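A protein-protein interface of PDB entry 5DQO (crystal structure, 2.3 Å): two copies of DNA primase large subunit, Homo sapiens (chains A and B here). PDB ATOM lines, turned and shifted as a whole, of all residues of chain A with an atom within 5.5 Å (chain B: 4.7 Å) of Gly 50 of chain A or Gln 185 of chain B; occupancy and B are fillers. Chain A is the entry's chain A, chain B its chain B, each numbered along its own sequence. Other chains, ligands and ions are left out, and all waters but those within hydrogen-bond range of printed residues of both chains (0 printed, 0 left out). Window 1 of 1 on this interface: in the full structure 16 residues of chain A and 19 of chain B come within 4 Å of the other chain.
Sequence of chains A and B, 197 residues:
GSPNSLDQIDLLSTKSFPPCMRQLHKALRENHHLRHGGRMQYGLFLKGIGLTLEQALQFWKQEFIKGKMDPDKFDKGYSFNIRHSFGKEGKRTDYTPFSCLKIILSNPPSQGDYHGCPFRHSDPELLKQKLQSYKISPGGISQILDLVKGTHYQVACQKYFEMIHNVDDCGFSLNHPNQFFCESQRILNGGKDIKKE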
ATOM      1  N   LEU A  46      18.051  12.153  -0.165  1.00  0.00           N
ATOM      2  CA  LEU A  46      18.497  11.179   0.746  1.00  0.00           C
ATOM      3  C   LEU A  46      19.025   9.950   0.042  1.00  0.00           C
ATOM      4  O   LEU A  46      20.037   9.332   0.460  1.00  0.00           O
ATOM      5  CB  LEU A  46      17.320  10.810   1.612  1.00  0.00           C
ATOM      6  CG  LEU A  46      16.935  11.989   2.474  1.00  0.00           C
ATOM      7  CD1 LEU A  46      15.712  11.548   3.270  1.00  0.00           C
ATOM      8  CD2 LEU A  46      18.080  12.325   3.417  1.00  0.00           C
ATOM      9  N   LYS A  47      18.357   9.558  -1.013  1.00  0.00           N
ATOM     10  CA  LYS A  47      18.854   8.476  -1.755  1.00  0.00           C
ATOM     11  C   LYS A  47      20.238   8.755  -2.283  1.00  0.00           C
ATOM     12  O   LYS A  47      21.085   7.852  -2.240  1.00  0.00           O
ATOM     13  CB  LYS A  47      17.868   8.087  -2.870  1.00  0.00           C
ATOM     14  N   GLY A  48      20.506   9.990  -2.713  1.00  0.00           N
ATOM     15  CA  GLY A  48      21.819  10.409  -3.131  1.00  0.00           C
ATOM     16  C   GLY A  48      22.908  10.228  -2.090  1.00  0.00           C
ATOM     17  O   GLY A  48      24.067  10.073  -2.433  1.00  0.00           O
ATOM     18  N   ILE A  49      22.521  10.264  -0.825  1.00  0.00           N
ATOM     19  CA  ILE A  49      23.382  10.037   0.329  1.00  0.00           C
ATOM     20  C   ILE A  49      23.654   8.540   0.576  1.00  0.00           C
ATOM     21  O   ILE A  49      24.619   8.200   1.256  1.00  0.00           O
ATOM     22  CB  ILE A  49      22.772  10.740   1.572  1.00  0.00           C
ATOM     23  CG1 ILE A  49      22.810  12.247   1.375  1.00  0.00           C
ATOM     24  CG2 ILE A  49      23.556  10.507   2.834  1.00  0.00           C
ATOM     25  CD1 ILE A  49      22.096  13.084   2.456  1.00  0.00           C
ATOM     26  N   GLY A  50      22.784   7.710   0.037  1.00  0.00           N
ATOM     27  CA  GLY A  50      22.886   6.309   0.202  1.00  0.00           C
ATOM     28  C   GLY A  50      21.903   5.837   1.207  1.00  0.00           C
ATOM     29  O   GLY A  50      21.924   4.704   1.546  1.00  0.00           O
ATOM     30  N   LEU A  51      21.017   6.694   1.662  1.00  0.00           N
ATOM     31  CA  LEU A  51      19.991   6.285   2.584  1.00  0.00           C
ATOM     32  C   LEU A  51      18.702   6.100   1.844  1.00  0.00           C
ATOM     33  O   LEU A  51      18.572   6.539   0.769  1.00  0.00           O
ATOM     34  CB  LEU A  51      19.778   7.362   3.591  1.00  0.00           C
ATOM     35  CG  LEU A  51      20.983   7.906   4.287  1.00  0.00           C
ATOM     36  CD1 LEU A  51      20.529   9.059   5.127  1.00  0.00           C
ATOM     37  CD2 LEU A  51      21.543   6.812   5.154  1.00  0.00           C
ATOM     38  N   THR A  52      17.741   5.453   2.455  1.00  0.00           N
ATOM     39  CA  THR A  52      16.444   5.273   1.840  1.00  0.00           C
ATOM     40  C   THR A  52      15.249   5.503   2.744  1.00  0.00           C
ATOM     41  O   THR A  52      14.929   4.675   3.488  1.00  0.00           O
ATOM     42  CB  THR A  52      16.298   3.867   1.285  1.00  0.00           C
ATOM     43  OG1 THR A  52      17.485   3.479   0.618  1.00  0.00           O
ATOM     44  CG2 THR A  52      15.187   3.815   0.365  1.00  0.00           C
ATOM     45  N   ARG A  83      16.941   4.082   6.094  1.00  0.00           N
ATOM     46  CA  ARG A  83      17.887   3.058   6.267  1.00  0.00           C
ATOM     47  C   ARG A  83      18.913   3.276   5.237  1.00  0.00           C
ATOM     48  O   ARG A  83      18.907   4.259   4.579  1.00  0.00           O
ATOM     49  CB  ARG A  83      17.213   1.738   6.008  1.00  0.00           C
ATOM     50  CG  ARG A  83      16.322   1.692   4.799  1.00  0.00           C
ATOM     51  CD  ARG A  83      16.187   0.266   4.364  1.00  0.00           C
ATOM     52  NE  ARG A  83      15.270   0.103   3.258  1.00  0.00           N
ATOM     53  CZ  ARG A  83      15.608  -0.175   1.998  1.00  0.00           C
ATOM     54  NH1 ARG A  83      16.868  -0.310   1.637  1.00  0.00           N
ATOM     55  NH2 ARG A  83      14.666  -0.313   1.086  1.00  0.00           N
ATOM     56  N   HIS A  84      19.791   2.312   5.098  1.00  0.00           N
ATOM     57  CA  HIS A  84      20.859   2.341   4.157  1.00  0.00           C
ATOM     58  C   HIS A  84      20.453   1.651   2.936  1.00  0.00           C
ATOM     59  O   HIS A  84      19.697   0.730   2.978  1.00  0.00           O
ATOM     60  CB  HIS A  84      22.020   1.597   4.717  1.00  0.00           C
ATOM     61  CG  HIS A  84      22.869   2.418   5.594  1.00  0.00           C
ATOM     62  ND1 HIS A  84      22.690   2.468   6.941  1.00  0.00           N
ATOM     63  CD2 HIS A  84      23.932   3.185   5.328  1.00  0.00           C
ATOM     64  CE1 HIS A  84      23.585   3.257   7.471  1.00  0.00           C
ATOM     65  NE2 HIS A  84      24.350   3.707   6.511  1.00  0.00           N
ATOM     66  N   SER A  85      20.985   2.097   1.829  1.00  0.00           N
ATOM     67  CA  SER A  85      20.664   1.527   0.576  1.00  0.00           C
ATOM     68  C   SER A  85      21.357   0.235   0.209  1.00  0.00           C
ATOM     69  O   SER A  85      20.849  -0.499  -0.593  1.00  0.00           O
ATOM     70  CB  SER A  85      20.945   2.543  -0.468  1.00  0.00           C
ATOM     71  OG  SER A  85      22.309   2.782  -0.437  1.00  0.00           O
ATOM     72  N   PHE A  86      22.514  -0.047   0.776  1.00  0.00           N
ATOM     73  CA  PHE A  86      23.213  -1.262   0.450  1.00  0.00           C
ATOM     74  C   PHE A  86      22.393  -2.412   0.999  1.00  0.00           C
ATOM     75  O   PHE A  86      21.873  -3.229   0.269  1.00  0.00           O
ATOM     76  CB  PHE A  86      24.597  -1.238   1.069  1.00  0.00           C
ATOM     77  CG  PHE A  86      24.581  -1.424   2.543  1.00  0.00           C
ATOM     78  CD1 PHE A  86      24.413  -2.647   3.077  1.00  0.00           C
ATOM     79  CD2 PHE A  86      24.699  -0.367   3.388  1.00  0.00           C
ATOM     80  CE1 PHE A  86      24.375  -2.816   4.420  1.00  0.00           C
ATOM     81  CE2 PHE A  86      24.673  -0.538   4.745  1.00  0.00           C
ATOM     82  CZ  PHE A  86      24.507  -1.771   5.255  1.00  0.00           C
ATOM     83  N   LEU B  12      29.429  -2.893  -1.356  1.00  0.00           N
ATOM     84  CA  LEU B  12      29.495  -1.503  -1.045  1.00  0.00           C
ATOM     85  C   LEU B  12      30.948  -1.122  -0.961  1.00  0.00           C
ATOM     86  O   LEU B  12      31.341  -0.051  -1.421  1.00  0.00           O
ATOM     87  CB  LEU B  12      28.821  -1.223   0.317  1.00  0.00           C
ATOM     88  CG  LEU B  12      28.580   0.254   0.500  1.00  0.00           C
ATOM     89  CD1 LEU B  12      27.391   0.664  -0.386  1.00  0.00           C
ATOM     90  CD2 LEU B  12      28.414   0.677   1.939  1.00  0.00           C
ATOM     91  N   SER B  16      32.091   1.487  -3.704  1.00  0.00           N
ATOM     92  CA  SER B  16      32.305   2.818  -3.174  1.00  0.00           C
ATOM     93  C   SER B  16      33.281   3.165  -2.077  1.00  0.00           C
ATOM     94  O   SER B  16      33.315   4.271  -1.644  1.00  0.00           O
ATOM     95  CB  SER B  16      30.981   3.360  -2.744  1.00  0.00           C
ATOM     96  OG  SER B  16      30.269   3.803  -3.824  1.00  0.00           O
ATOM     97  N   PHE B 181      33.630   8.379  -0.294  1.00  0.00           N
ATOM     98  CA  PHE B 181      32.396   7.655  -0.115  1.00  0.00           C
ATOM     99  C   PHE B 181      31.156   8.344  -0.636  1.00  0.00           C
ATOM    100  O   PHE B 181      30.427   7.707  -1.356  1.00  0.00           O
ATOM    101  CB  PHE B 181      32.204   7.156   1.304  1.00  0.00           C
ATOM    102  CG  PHE B 181      31.100   6.190   1.429  1.00  0.00           C
ATOM    103  CD1 PHE B 181      31.280   4.885   1.094  1.00  0.00           C
ATOM    104  CD2 PHE B 181      29.873   6.587   1.823  1.00  0.00           C
ATOM    105  CE1 PHE B 181      30.256   3.991   1.186  1.00  0.00           C
ATOM    106  CE2 PHE B 181      28.844   5.699   1.904  1.00  0.00           C
ATOM    107  CZ  PHE B 181      29.034   4.398   1.597  1.00  0.00           C
ATOM    108  N   CYS B 182      30.907   9.574  -0.202  1.00  0.00           N
ATOM    109  CA  CYS B 182      29.709  10.307  -0.592  1.00  0.00           C
ATOM    110  C   CYS B 182      29.794  10.855  -2.000  1.00  0.00           C
ATOM    111  O   CYS B 182      28.774  11.171  -2.613  1.00  0.00           O
ATOM    112  CB  CYS B 182      29.438  11.447   0.396  1.00  0.00           C
ATOM    113  SG  CYS B 182      28.326  12.727  -0.229  1.00  0.00           S
ATOM    114  N   GLU B 183      31.010  10.969  -2.517  1.00  0.00           N
ATOM    115  CA  GLU B 183      31.170  11.474  -3.820  1.00  0.00           C
ATOM    116  C   GLU B 183      30.964  10.334  -4.756  1.00  0.00           C
ATOM    117  O   GLU B 183      30.797  10.549  -5.899  1.00  0.00           O
ATOM    118  CB  GLU B 183      32.518  12.086  -4.002  1.00  0.00           C
ATOM    119  CG  GLU B 183      32.678  13.358  -3.238  1.00  0.00           C
ATOM    120  CD  GLU B 183      32.112  14.562  -3.938  1.00  0.00           C
ATOM    121  OE1 GLU B 183      31.129  14.422  -4.657  1.00  0.00           O
ATOM    122  OE2 GLU B 183      32.646  15.649  -3.756  1.00  0.00           O
ATOM    123  N   SER B 184      30.969   9.123  -4.244  1.00  0.00           N
ATOM    124  CA  SER B 184      30.748   7.957  -4.958  1.00  0.00           C
ATOM    125  C   SER B 184      29.302   7.675  -4.823  1.00  0.00           C
ATOM    126  O   SER B 184      28.679   7.396  -5.803  1.00  0.00           O
ATOM    127  CB  SER B 184      31.553   6.825  -4.345  1.00  0.00           C
ATOM    128  OG  SER B 184      31.476   5.681  -5.135  1.00  0.00           O
ATOM    129  N   GLN B 185      28.775   7.743  -3.618  1.00  0.00           N
ATOM    130  CA  GLN B 185      27.391   7.431  -3.445  1.00  0.00           C
ATOM    131  C   GLN B 185      26.536   8.266  -4.318  1.00  0.00           C
ATOM    132  O   GLN B 185      25.515   7.812  -4.728  1.00  0.00           O
ATOM    133  CB  GLN B 185      26.936   7.368  -2.011  1.00  0.00           C
ATOM    134  CG  GLN B 185      27.224   6.025  -1.349  1.00  0.00           C
ATOM    135  CD  GLN B 185      26.575   4.799  -1.981  1.00  0.00           C
ATOM    136  OE1 GLN B 185      27.024   4.315  -2.969  1.00  0.00           O
ATOM    137  NE2 GLN B 185      25.518   4.349  -1.430  1.00  0.00           N
ATOM    138  N   ARG B 186      26.973   9.473  -4.627  1.00  0.00           N
ATOM    139  CA  ARG B 186      26.247  10.379  -5.504  1.00  0.00           C
ATOM    140  C   ARG B 186      26.070   9.880  -6.908  1.00  0.00           C
ATOM    141  O   ARG B 186      25.004   9.938  -7.447  1.00  0.00           O
ATOM    142  CB  ARG B 186      26.919  11.714  -5.569  1.00  0.00           C
ATOM    143  CG  ARG B 186      26.535  12.666  -4.474  1.00  0.00           C
ATOM    144  CD  ARG B 186      27.308  13.946  -4.556  1.00  0.00           C
ATOM    145  NE  ARG B 186      26.682  14.880  -5.463  1.00  0.00           N
ATOM    146  CZ  ARG B 186      27.334  15.796  -6.129  1.00  0.00           C
ATOM    147  NH1 ARG B 186      28.615  15.912  -5.987  1.00  0.00           N
ATOM    148  NH2 ARG B 186      26.695  16.586  -6.917  1.00  0.00           N
ATOM    149  N   ILE B 187      27.140   9.401  -7.493  1.00  0.00           N
ATOM    150  CA  ILE B 187      27.118   8.836  -8.822  1.00  0.00           C
ATOM    151  C   ILE B 187      26.305   7.573  -8.907  1.00  0.00           C
ATOM    152  O   ILE B 187      25.653   7.362  -9.885  1.00  0.00           O
ATOM    153  CB  ILE B 187      28.558   8.567  -9.323  1.00  0.00           C
ATOM    154  CG1 ILE B 187      29.146   9.810  -9.924  1.00  0.00           C
ATOM    155  CG2 ILE B 187      28.676   7.556 -10.428  1.00  0.00           C
ATOM    156  CD1 ILE B 187      30.590   9.984  -9.588  1.00  0.00           C
ATOM    157  N   LEU B 188      26.381   6.740  -7.904  1.00  0.00           N
ATOM    158  CA  LEU B 188      25.717   5.479  -7.974  1.00  0.00           C
ATOM    159  C   LEU B 188      24.250   5.531  -7.864  1.00  0.00           C
ATOM    160  O   LEU B 188      23.549   4.941  -8.631  1.00  0.00           O
ATOM    161  CB  LEU B 188      26.353   4.496  -7.029  1.00  0.00           C
ATOM    162  CG  LEU B 188      27.841   4.444  -7.289  1.00  0.00           C
ATOM    163  CD1 LEU B 188      28.485   3.376  -6.490  1.00  0.00           C
ATOM    164  CD2 LEU B 188      28.141   4.188  -8.730  1.00  0.00           C
ATOM    165  N   ASN B 189      23.776   6.254  -6.905  1.00  0.00           N
ATOM    166  CA  ASN B 189      22.359   6.369  -6.692  1.00  0.00           C
ATOM    167  C   ASN B 189      21.879   7.546  -7.470  1.00  0.00           C
ATOM    168  O   ASN B 189      20.906   8.140  -7.119  1.00  0.00           O
ATOM    169  CB  ASN B 189      22.043   6.526  -5.213  1.00  0.00           C
ATOM    170  CG  ASN B 189      23.022   5.823  -4.348  1.00  0.00           C
ATOM    171  OD1 ASN B 189      23.498   6.388  -3.421  1.00  0.00           O
ATOM    172  ND2 ASN B 189      23.231   4.573  -4.582  1.00  0.00           N
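O of Gly 50 of chain A lies within hydrogen-bond range of N of Ser 85 of chain A, 2.8 Å away. The side-chain amide oxygen (OE1) of Gln 185 of chain B lies within hydrogen-bond range of the side-chain hydroxyl (OG) of Ser 16 of chain B (3.4 Å). The guanidinium group (NH1) of Arg 186 of chain B is in salt-bridge range of the side-chain carboxylate (OE1) of Glu 183 of chain B, at 3.2 Å. O of Gln 185 of chain B lies close to OD1 of Asn 189 of chain B, at 2.8 Å.
Among the printed residues, merely in contact across the chains: Gly 48 of chain A with Gln 185 of chain B, Gly 50 of chain A with Gln 185 of chain B, Gly 50 of chain A with Asn 189 of chain B, Phe 86 of chain A with Leu 12 of chain B, Gly 48 of chain A with Arg 186 of chain B, Ser 85 of chain A with Gln 185 of chain B and Gly 48 of chain A with Asn 189 of chain B.
Gly 50 of chain A touches just these residues of chain B: Gln 185 and Asn 189. Gln 185 of chain B touches just these residues of chain A: Gly 48 (3.5 Å), Gly 50 (3.7 Å) and Ser 85 (3.7 Å). Of the printed residues of chain B, Gly 48 of chain A touches Gln 185 (3.5 Å), Arg 186 (3.7 Å) and Asn 189 (3.9 Å). Printed residues of chain A within 4 Å of Leu 12 of chain B: Phe 86 (3.7 Å). Printed residues of chain A within 4 Å of Arg 186 of chain B: Gly 48. Cys 182 of chain B touches none of the printed residues of chain A. Ile 49 of chain A touches none of the printed residues of chain B.
O of Lys 47 of chain A sits close to OD1 of Asn 189 of chain B, at 3.1 Å.
No position is printed for both chains. Of the 8 pairs that touch across the chains among the printed residues, none has its exchanged pair printed and touching as well.
Printed residues of chain B that touch a printed residue of chain A: Leu 12, Gln 185, Arg 186 and Asn 189. Among the printed residues, 8 pairs touch across the chains. Among the printed residues, no Asp or Glu carboxylate lies within 4 Å of a Lys or Arg side-chain nitrogen of the other chain.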
